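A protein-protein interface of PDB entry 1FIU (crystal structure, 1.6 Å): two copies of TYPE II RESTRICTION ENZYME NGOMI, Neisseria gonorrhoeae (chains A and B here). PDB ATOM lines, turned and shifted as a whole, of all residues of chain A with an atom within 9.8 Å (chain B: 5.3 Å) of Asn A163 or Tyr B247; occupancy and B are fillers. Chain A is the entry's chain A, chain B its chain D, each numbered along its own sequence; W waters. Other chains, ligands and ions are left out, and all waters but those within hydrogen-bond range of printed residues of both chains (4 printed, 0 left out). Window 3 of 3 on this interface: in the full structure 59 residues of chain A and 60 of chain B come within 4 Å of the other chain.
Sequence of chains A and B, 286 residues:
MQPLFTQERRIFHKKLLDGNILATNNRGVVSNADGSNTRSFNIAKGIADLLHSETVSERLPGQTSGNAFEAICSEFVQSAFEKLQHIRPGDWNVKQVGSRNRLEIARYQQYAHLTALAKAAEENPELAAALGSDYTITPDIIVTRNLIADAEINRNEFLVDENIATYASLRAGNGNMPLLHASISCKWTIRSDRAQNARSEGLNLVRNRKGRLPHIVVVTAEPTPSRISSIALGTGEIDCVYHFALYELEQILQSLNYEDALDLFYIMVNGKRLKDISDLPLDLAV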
ATOM      1  N   ASP A 150     -31.256 -23.817  19.013  1.00  0.00           N
ATOM      2  CA  ASP A 150     -30.879 -22.428  18.815  1.00  0.00           C
ATOM      3  C   ASP A 150     -31.327 -21.580  20.016  1.00  0.00           C
ATOM      4  O   ASP A 150     -30.657 -20.625  20.397  1.00  0.00           O
ATOM      5  CB  ASP A 150     -31.513 -21.901  17.524  1.00  0.00           C
ATOM      6  CG  ASP A 150     -30.792 -22.381  16.286  1.00  0.00           C
ATOM      7  OD1 ASP A 150     -29.841 -23.182  16.419  1.00  0.00           O
ATOM      8  OD2 ASP A 150     -31.185 -21.947  15.184  1.00  0.00           O
ATOM      9  N   PHE A 158     -29.695 -12.720  21.519  1.00  0.00           N
ATOM     10  CA  PHE A 158     -29.954 -13.199  20.169  1.00  0.00           C
ATOM     11  C   PHE A 158     -28.603 -13.325  19.435  1.00  0.00           C
ATOM     12  O   PHE A 158     -28.147 -12.378  18.806  1.00  0.00           O
ATOM     13  CB  PHE A 158     -30.855 -12.200  19.427  1.00  0.00           C
ATOM     14  CG  PHE A 158     -31.178 -12.591  18.004  1.00  0.00           C
ATOM     15  CD1 PHE A 158     -31.378 -13.918  17.645  1.00  0.00           C
ATOM     16  CD2 PHE A 158     -31.313 -11.604  17.019  1.00  0.00           C
ATOM     17  CE1 PHE A 158     -31.713 -14.272  16.325  1.00  0.00           C
ATOM     18  CE2 PHE A 158     -31.647 -11.958  15.691  1.00  0.00           C
ATOM     19  CZ  PHE A 158     -31.843 -13.289  15.356  1.00  0.00           C
ATOM     20  N   LEU A 159     -27.988 -14.501  19.532  1.00  0.00           N
ATOM     21  CA  LEU A 159     -26.671 -14.762  18.935  1.00  0.00           C
ATOM     22  C   LEU A 159     -26.690 -15.331  17.519  1.00  0.00           C
ATOM     23  O   LEU A 159     -25.868 -14.944  16.688  1.00  0.00           O
ATOM     24  CB  LEU A 159     -25.864 -15.712  19.833  1.00  0.00           C
ATOM     25  CG  LEU A 159     -25.651 -15.336  21.305  1.00  0.00           C
ATOM     26  CD1 LEU A 159     -24.724 -16.380  21.966  1.00  0.00           C
ATOM     27  CD2 LEU A 159     -25.047 -13.937  21.409  1.00  0.00           C
ATOM     28  N   VAL A 160     -27.600 -16.257  17.244  1.00  0.00           N
ATOM     29  CA  VAL A 160     -27.658 -16.871  15.924  1.00  0.00           C
ATOM     30  C   VAL A 160     -29.074 -17.066  15.352  1.00  0.00           C
ATOM     31  O   VAL A 160     -30.065 -17.122  16.090  1.00  0.00           O
ATOM     32  CB  VAL A 160     -26.997 -18.298  15.921  1.00  0.00           C
ATOM     33  CG1 VAL A 160     -25.531 -18.218  16.419  1.00  0.00           C
ATOM     34  CG2 VAL A 160     -27.826 -19.282  16.805  1.00  0.00           C
ATOM     35  N   ASP A 161     -29.136 -17.120  14.020  1.00  0.00           N
ATOM     36  CA  ASP A 161     -30.372 -17.465  13.317  1.00  0.00           C
ATOM     37  C   ASP A 161     -29.949 -18.511  12.281  1.00  0.00           C
ATOM     38  O   ASP A 161     -28.834 -19.028  12.369  1.00  0.00           O
ATOM     39  CB  ASP A 161     -31.081 -16.237  12.703  1.00  0.00           C
ATOM     40  CG  ASP A 161     -30.341 -15.602  11.549  1.00  0.00           C
ATOM     41  OD1 ASP A 161     -29.249 -16.049  11.122  1.00  0.00           O
ATOM     42  OD2 ASP A 161     -30.896 -14.596  11.058  1.00  0.00           O
ATOM     43  N   GLU A 162     -30.797 -18.845  11.308  1.00  0.00           N
ATOM     44  CA  GLU A 162     -30.450 -19.890  10.339  1.00  0.00           C
ATOM     45  C   GLU A 162     -29.432 -19.543   9.252  1.00  0.00           C
ATOM     46  O   GLU A 162     -29.050 -20.416   8.468  1.00  0.00           O
ATOM     47  CB  GLU A 162     -31.721 -20.403   9.633  1.00  0.00           C
ATOM     48  CG  GLU A 162     -32.299 -19.416   8.617  1.00  0.00           C
ATOM     49  CD  GLU A 162     -33.260 -18.391   9.214  1.00  0.00           C
ATOM     50  OE1 GLU A 162     -33.315 -18.210  10.460  1.00  0.00           O
ATOM     51  OE2 GLU A 162     -33.972 -17.744   8.413  1.00  0.00           O
ATOM     52  N   ASN A 163     -28.988 -18.292   9.211  1.00  0.00           N
ATOM     53  CA  ASN A 163     -28.048 -17.859   8.187  1.00  0.00           C
ATOM     54  C   ASN A 163     -26.638 -17.517   8.666  1.00  0.00           C
ATOM     55  O   ASN A 163     -25.865 -16.942   7.905  1.00  0.00           O
ATOM     56  CB  ASN A 163     -28.616 -16.646   7.450  1.00  0.00           C
ATOM     57  CG  ASN A 163     -29.938 -16.951   6.785  1.00  0.00           C
ATOM     58  OD1 ASN A 163     -30.069 -17.947   6.090  1.00  0.00           O
ATOM     59  ND2 ASN A 163     -30.917 -16.090   6.996  1.00  0.00           N
ATOM     60  N   ILE A 164     -26.314 -17.865   9.906  1.00  0.00           N
ATOM     61  CA  ILE A 164     -24.981 -17.583  10.472  1.00  0.00           C
ATOM     62  C   ILE A 164     -24.546 -18.806  11.285  1.00  0.00           C
ATOM     63  O   ILE A 164     -25.396 -19.499  11.825  1.00  0.00           O
ATOM     64  CB  ILE A 164     -25.039 -16.328  11.376  1.00  0.00           C
ATOM     65  CG1 ILE A 164     -23.633 -15.912  11.832  1.00  0.00           C
ATOM     66  CG2 ILE A 164     -25.948 -16.570  12.579  1.00  0.00           C
ATOM     67  CD1 ILE A 164     -22.813 -15.192  10.760  1.00  0.00           C
ATOM     68  N   ALA A 165     -23.233 -19.082  11.355  1.00  0.00           N
ATOM     69  CA  ALA A 165     -22.727 -20.231  12.126  1.00  0.00           C
ATOM     70  C   ALA A 165     -23.490 -21.492  11.756  1.00  0.00           C
ATOM     71  O   ALA A 165     -23.882 -22.306  12.622  1.00  0.00           O
ATOM     72  CB  ALA A 165     -22.862 -19.951  13.638  1.00  0.00           C
ATOM     73  N   THR A 166     -23.661 -21.665  10.448  1.00  0.00           N
ATOM     74  CA  THR A 166     -24.451 -22.769   9.925  1.00  0.00           C
ATOM     75  C   THR A 166     -23.845 -24.152   9.945  1.00  0.00           C
ATOM     76  O   THR A 166     -24.562 -25.142   9.720  1.00  0.00           O
ATOM     77  CB  THR A 166     -24.937 -22.455   8.490  1.00  0.00           C
ATOM     78  OG1 THR A 166     -23.821 -22.421   7.600  1.00  0.00           O
ATOM     79  CG2 THR A 166     -25.629 -21.103   8.450  1.00  0.00           C
ATOM     80  N   TYR A 167     -22.549 -24.247  10.262  1.00  0.00           N
ATOM     81  CA  TYR A 167     -21.879 -25.545  10.310  1.00  0.00           C
ATOM     82  C   TYR A 167     -21.375 -25.870  11.711  1.00  0.00           C
ATOM     83  O   TYR A 167     -20.662 -26.870  11.891  1.00  0.00           O
ATOM     84  CB  TYR A 167     -20.693 -25.567   9.324  1.00  0.00           C
ATOM     85  CG  TYR A 167     -21.133 -25.383   7.877  1.00  0.00           C
ATOM     86  CD1 TYR A 167     -20.819 -24.227   7.187  1.00  0.00           C
ATOM     87  CD2 TYR A 167     -21.899 -26.350   7.234  1.00  0.00           C
ATOM     88  CE1 TYR A 167     -21.254 -24.022   5.885  1.00  0.00           C
ATOM     89  CE2 TYR A 167     -22.339 -26.155   5.930  1.00  0.00           C
ATOM     90  CZ  TYR A 167     -22.010 -24.987   5.272  1.00  0.00           C
ATOM     91  OH  TYR A 167     -22.448 -24.762   3.988  1.00  0.00           O
ATOM     92  N   ALA A 168     -21.747 -25.045  12.686  1.00  0.00           N
ATOM     93  CA  ALA A 168     -21.299 -25.247  14.075  1.00  0.00           C
ATOM     94  C   ALA A 168     -21.697 -26.642  14.548  1.00  0.00           C
ATOM     95  O   ALA A 168     -22.861 -27.043  14.465  1.00  0.00           O
ATOM     96  CB  ALA A 168     -21.910 -24.199  14.994  1.00  0.00           C
ATOM     97  N   ARG A 171     -24.880 -27.362  16.789  1.00  0.00           N
ATOM     98  CA  ARG A 171     -26.254 -27.107  16.372  1.00  0.00           C
ATOM     99  C   ARG A 171     -26.989 -28.315  15.859  1.00  0.00           C
ATOM    100  O   ARG A 171     -26.518 -29.034  14.995  1.00  0.00           O
ATOM    101  CB  ARG A 171     -26.286 -25.944  15.374  1.00  0.00           C
ATOM    102  CG  ARG A 171     -25.868 -24.669  16.079  1.00  0.00           C
ATOM    103  CD  ARG A 171     -25.861 -23.462  15.167  1.00  0.00           C
ATOM    104  NE  ARG A 171     -27.221 -22.965  14.937  1.00  0.00           N
ATOM    105  CZ  ARG A 171     -27.485 -21.938  14.144  1.00  0.00           C
ATOM    106  NH1 ARG A 171     -26.478 -21.334  13.520  1.00  0.00           N
ATOM    107  NH2 ARG A 171     -28.732 -21.505  13.996  1.00  0.00           N
ATOM    108  N   MET B   1     -27.483  -8.474   9.194  1.00  0.00           N
ATOM    109  CA  MET B   1     -28.637  -8.920  10.016  1.00  0.00           C
ATOM    110  C   MET B   1     -28.478  -8.443  11.435  1.00  0.00           C
ATOM    111  O   MET B   1     -27.626  -7.614  11.740  1.00  0.00           O
ATOM    112  CB  MET B   1     -28.758 -10.451  10.003  1.00  0.00           C
ATOM    113  CG  MET B   1     -29.262 -11.002   8.680  1.00  0.00           C
ATOM    114  SD  MET B   1     -29.646 -12.761   8.721  1.00  0.00           S
ATOM    115  CE  MET B   1     -28.661 -13.357   7.327  1.00  0.00           C
ATOM    116  N   ARG B   9     -19.385 -10.886  12.949  1.00  0.00           N
ATOM    117  CA  ARG B   9     -18.729 -11.295  11.713  1.00  0.00           C
ATOM    118  C   ARG B   9     -18.527 -10.062  10.829  1.00  0.00           C
ATOM    119  O   ARG B   9     -17.466  -9.882  10.240  1.00  0.00           O
ATOM    120  CB  ARG B   9     -19.583 -12.337  10.995  1.00  0.00           C
ATOM    121  CG  ARG B   9     -19.005 -12.840   9.664  1.00  0.00           C
ATOM    122  CD  ARG B   9     -19.975 -13.862   9.074  1.00  0.00           C
ATOM    123  NE  ARG B   9     -19.420 -14.637   7.957  1.00  0.00           N
ATOM    124  CZ  ARG B   9     -19.452 -14.274   6.679  1.00  0.00           C
ATOM    125  NH1 ARG B   9     -20.026 -13.111   6.314  1.00  0.00           N
ATOM    126  NH2 ARG B   9     -18.923 -15.086   5.767  1.00  0.00           N
ATOM    127  N   ALA B 245     -14.623 -15.622   4.900  1.00  0.00           N
ATOM    128  CA  ALA B 245     -15.835 -15.164   4.186  1.00  0.00           C
ATOM    129  C   ALA B 245     -16.394 -16.346   3.384  1.00  0.00           C
ATOM    130  O   ALA B 245     -16.457 -16.309   2.151  1.00  0.00           O
ATOM    131  CB  ALA B 245     -15.476 -13.982   3.238  1.00  0.00           C
ATOM    132  N   LEU B 246     -16.804 -17.399   4.084  1.00  0.00           N
ATOM    133  CA  LEU B 246     -17.246 -18.605   3.395  1.00  0.00           C
ATOM    134  C   LEU B 246     -18.483 -18.446   2.517  1.00  0.00           C
ATOM    135  O   LEU B 246     -18.517 -18.988   1.403  1.00  0.00           O
ATOM    136  CB  LEU B 246     -17.500 -19.740   4.405  1.00  0.00           C
ATOM    137  CG  LEU B 246     -17.616 -21.126   3.750  1.00  0.00           C
ATOM    138  CD1 LEU B 246     -16.218 -21.729   3.539  1.00  0.00           C
ATOM    139  CD2 LEU B 246     -18.447 -22.059   4.663  1.00  0.00           C
ATOM    140  N   TYR B 247     -19.486 -17.712   3.007  1.00  0.00           N
ATOM    141  CA  TYR B 247     -20.730 -17.591   2.221  1.00  0.00           C
ATOM    142  C   TYR B 247     -20.476 -16.844   0.929  1.00  0.00           C
ATOM    143  O   TYR B 247     -21.037 -17.192  -0.128  1.00  0.00           O
ATOM    144  CB  TYR B 247     -21.799 -16.860   3.023  1.00  0.00           C
ATOM    145  CG  TYR B 247     -21.903 -17.356   4.453  1.00  0.00           C
ATOM    146  CD1 TYR B 247     -22.032 -16.447   5.498  1.00  0.00           C
ATOM    147  CD2 TYR B 247     -21.872 -18.710   4.749  1.00  0.00           C
ATOM    148  CE1 TYR B 247     -22.125 -16.879   6.818  1.00  0.00           C
ATOM    149  CE2 TYR B 247     -21.969 -19.159   6.079  1.00  0.00           C
ATOM    150  CZ  TYR B 247     -22.092 -18.231   7.092  1.00  0.00           C
ATOM    151  OH  TYR B 247     -22.178 -18.627   8.408  1.00  0.00           O
ATOM    152  N   GLU B 248     -19.614 -15.846   1.020  1.00  0.00           N
ATOM    153  CA  GLU B 248     -19.256 -15.007  -0.138  1.00  0.00           C
ATOM    154  C   GLU B 248     -18.431 -15.829  -1.132  1.00  0.00           C
ATOM    155  O   GLU B 248     -18.608 -15.717  -2.350  1.00  0.00           O
ATOM    156  CB  GLU B 248     -18.468 -13.766   0.319  1.00  0.00           C
ATOM    157  CG  GLU B 248     -19.270 -12.780   1.190  1.00  0.00           C
ATOM    158  CD  GLU B 248     -19.422 -13.207   2.651  1.00  0.00           C
ATOM    159  OE1 GLU B 248     -18.855 -14.252   3.040  1.00  0.00           O
ATOM    160  OE2 GLU B 248     -20.113 -12.487   3.412  1.00  0.00           O
ATOM    161  N   LEU B 249     -17.497 -16.635  -0.613  1.00  0.00           N
ATOM    162  CA  LEU B 249     -16.693 -17.499  -1.454  1.00  0.00           C
ATOM    163  C   LEU B 249     -17.613 -18.439  -2.254  1.00  0.00           C
ATOM    164  O   LEU B 249     -17.472 -18.582  -3.466  1.00  0.00           O
ATOM    165  CB  LEU B 249     -15.718 -18.333  -0.587  1.00  0.00           C
ATOM    166  CG  LEU B 249     -14.925 -19.449  -1.289  1.00  0.00           C
ATOM    167  CD1 LEU B 249     -14.090 -18.878  -2.460  1.00  0.00           C
ATOM    168  CD2 LEU B 249     -13.993 -20.137  -0.259  1.00  0.00           C
ATOM    169  N   GLU B 250     -18.569 -19.070  -1.579  1.00  0.00           N
ATOM    170  CA  GLU B 250     -19.487 -19.989  -2.256  1.00  0.00           C
ATOM    171  C   GLU B 250     -20.262 -19.251  -3.334  1.00  0.00           C
ATOM    172  O   GLU B 250     -20.387 -19.736  -4.470  1.00  0.00           O
ATOM    173  CB  GLU B 250     -20.478 -20.600  -1.248  1.00  0.00           C
ATOM    174  CG  GLU B 250     -21.442 -21.610  -1.850  1.00  0.00           C
ATOM    175  CD  GLU B 250     -22.472 -22.115  -0.824  1.00  0.00           C
ATOM    176  OE1 GLU B 250     -22.696 -21.427   0.200  1.00  0.00           O
ATOM    177  OE2 GLU B 250     -23.070 -23.191  -1.055  1.00  0.00           O
ATOM    178  N   GLN B 251     -20.779 -18.089  -2.986  1.00  0.00           N
ATOM    179  CA  GLN B 251     -21.567 -17.327  -3.958  1.00  0.00           C
ATOM    180  C   GLN B 251     -20.778 -16.942  -5.207  1.00  0.00           C
ATOM    181  O   GLN B 251     -21.274 -17.080  -6.341  1.00  0.00           O
ATOM    182  CB  GLN B 251     -22.150 -16.086  -3.303  1.00  0.00           C
ATOM    183  CG  GLN B 251     -23.195 -15.405  -4.198  1.00  0.00           C
ATOM    184  CD  GLN B 251     -23.823 -14.200  -3.534  1.00  0.00           C
ATOM    185  OE1 GLN B 251     -24.090 -14.215  -2.327  1.00  0.00           O
ATOM    186  NE2 GLN B 251     -24.071 -13.145  -4.315  1.00  0.00           N
ATOM    187  N   ILE B 252     -19.545 -16.486  -5.019  1.00  0.00           N
ATOM    188  CA  ILE B 252     -18.743 -16.084  -6.165  1.00  0.00           C
ATOM    189  C   ILE B 252     -18.312 -17.285  -7.011  1.00  0.00           C
ATOM    190  O   ILE B 252     -18.255 -17.192  -8.232  1.00  0.00           O
ATOM    191  CB  ILE B 252     -17.517 -15.214  -5.729  1.00  0.00           C
ATOM    192  CG1 ILE B 252     -16.846 -14.614  -6.968  1.00  0.00           C
ATOM    193  CG2 ILE B 252     -16.477 -16.032  -4.984  1.00  0.00           C
ATOM    194  CD1 ILE B 252     -17.793 -13.768  -7.859  1.00  0.00           C
ATOM    195  N   ASP B 276     -17.188 -21.581   8.218  1.00  0.00           N
ATOM    196  CA  ASP B 276     -17.068 -20.125   8.181  1.00  0.00           C
ATOM    197  C   ASP B 276     -16.450 -19.630   9.498  1.00  0.00           C
ATOM    198  O   ASP B 276     -16.537 -20.307  10.524  1.00  0.00           O
ATOM    199  CB  ASP B 276     -18.466 -19.489   8.046  1.00  0.00           C
ATOM    200  CG  ASP B 276     -18.410 -17.992   7.896  1.00  0.00           C
ATOM    201  OD1 ASP B 276     -17.871 -17.522   6.871  1.00  0.00           O
ATOM    202  OD2 ASP B 276     -18.886 -17.258   8.794  1.00  0.00           O
ATOM    203  N   SER B 278     -17.644 -17.610  11.403  1.00  0.00           N
ATOM    204  CA  SER B 278     -18.715 -17.525  12.408  1.00  0.00           C
ATOM    205  C   SER B 278     -19.010 -18.842  13.126  1.00  0.00           C
ATOM    206  O   SER B 278     -19.667 -18.844  14.178  1.00  0.00           O
ATOM    207  CB  SER B 278     -20.019 -16.981  11.784  1.00  0.00           C
ATOM    208  OG  SER B 278     -20.545 -17.909  10.854  1.00  0.00           O
ATOM    209  N   ASP B 279     -18.515 -19.955  12.592  1.00  0.00           N
ATOM    210  CA  ASP B 279     -18.706 -21.256  13.230  1.00  0.00           C
ATOM    211  C   ASP B 279     -17.684 -21.486  14.325  1.00  0.00           C
ATOM    212  O   ASP B 279     -17.908 -22.299  15.221  1.00  0.00           O
ATOM    213  CB  ASP B 279     -18.553 -22.396  12.218  1.00  0.00           C
ATOM    214  CG  ASP B 279     -19.647 -22.397  11.184  1.00  0.00           C
ATOM    215  OD1 ASP B 279     -20.811 -22.543  11.584  1.00  0.00           O
ATOM    216  OD2 ASP B 279     -19.346 -22.244   9.978  1.00  0.00           O
HETATM  217  O   HOH W   1     -22.037 -21.823   2.849  1.00  0.00           O
HETATM  218  O   HOH W   2     -21.443 -21.237   8.580  1.00  0.00           O
HETATM  219  O   HOH W   3     -31.590 -14.285   8.527  1.00  0.00           O
HETATM  220  O   HOH W   4     -27.635 -13.961  10.118  1.00  0.00           O
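Printed residues of chain B that touch a printed residue of chain A: Met B1, Arg B9, Leu B246, Tyr B247, Ser B278 and Asp B279. Hydrophobic or aromatic side chains of chain B that line the printed part of chain A: Met B1, Leu B246 and Tyr B247. Printed residues of chain A that touch a printed residue of chain B: Asp A161, Asn A163, Ile A164, Ala A165, Thr A166, Tyr A167 and Ala A168. Among the printed residues, no Asp or Glu carboxylate lies within 4 Å of a Lys or Arg side-chain nitrogen of the other chain.
Asn A163 touches two residues of chain B. Of the printed residues of chain B, Tyr A167 touches Leu B246 and Asp B279. Of the printed residues of chain B, Ala A168 touches Asp B279 (2.9 Å). Printed residues of chain A within 4 Å of Met B1: Asp A161 (3.2 Å) and Asn A163 (3.3 Å). Printed residues of chain A within 4 Å of Arg B9: Ile A164. No residue of chain A comes within 4 Å of Ala B245. Leu B246 touches one residue of chain A. Of chain A, only Asn A163 (3.9 Å), Ile A164 (3.6 Å), Ala A165 (3.2 Å) and Thr A166 (3.9 Å) come within 4 Å of Tyr B247. No residue of chain A comes within 4 Å of Glu B248. The nearest residue of chain A that does not touch Tyr B247 is Tyr A167 (4.9 Å).
Water W3 lies within hydrogen-bond range of the side-chain amide nitrogen of Asn A163, the side-chain sulfur of Met B1 and the side-chain carboxylate of Asp A161. Water W2 lies within hydrogen-bond range of the side-chain carboxylate of Asp B279 (2.7 Å), the side-chain hydroxyl of Tyr B247 (2.7 Å) and the side-chain hydroxyl of Thr A166 (2.8 Å). Water W4 lies within hydrogen-bond range of SD of Met B1 and OD1 of Asp A161. Water W1 lies within hydrogen-bond range of OE1 of Glu B250 (2.8 Å) and OH of Tyr A167 (3.2 Å).
Among the printed residues, merely in contact across the chains: Asn A163 with Met B1 (3.3 Å), Ile A164 with Ser B278 (3.5 Å), Ile A164 with Arg B9 (3.6 Å), Ile A164 with Tyr B247 (3.6 Å), Tyr A167 with Leu B246 (3.6 Å), Asn A163 with Tyr B247 (3.9 Å) and Thr A166 with Tyr B247 (3.9 Å).
No position is printed for both chains. Of the 14 pairs that touch across the chains among the printed residues, none has its exchanged pair printed and touching as well.
N of Ala A165 is in hydrogen-bond range of OH of Tyr B247 (3.2 Å). The side-chain hydroxyl (OG) of Ser B278 sits at hydrogen-bond distance from the backbone NH (N) of Ala A165 (3.0 Å). The side-chain carboxylate (OD1) of Asp B279 lies within hydrogen-bond range of the backbone NH (N) of Thr A166 (3.2 Å). N of Tyr A167 lies within hydrogen-bond range of OD1 of Asp B279 (2.8 Å). The backbone NH of Ala A168 is in hydrogen-bond range of the side-chain carboxylate of Asp B279, 2.9 Å away. The side-chain carboxylate (OD2) of Asp A161 sits close to the side-chain sulfur (SD) of Met B1 (3.2 Å). O of Ala A165 lies close to OD1 of Asp B279 (3.3 Å).
NH2 of Arg A171 sits at hydrogen-bond distance from O of Asp A161, 3.0 Å away. O of Ile A164 sits at hydrogen-bond distance from NH1 of Arg A171 (2.7 Å). The guanidinium group (NH1) of Arg A171 lies within hydrogen-bond range of the backbone carbonyl oxygen (O) of Ala A165, 2.9 Å away. The side-chain carboxylate of Glu B248 is in salt-bridge range of the guanidinium group of Arg B9 (2.9 Å). The guanidinium group (NE) of Arg B9 is in salt-bridge range of the side-chain carboxylate (OD2) of Asp B276. The backbone NH (N) of Leu B246 is in hydrogen-bond range of the side-chain carboxylate (OD1) of Asp B276.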
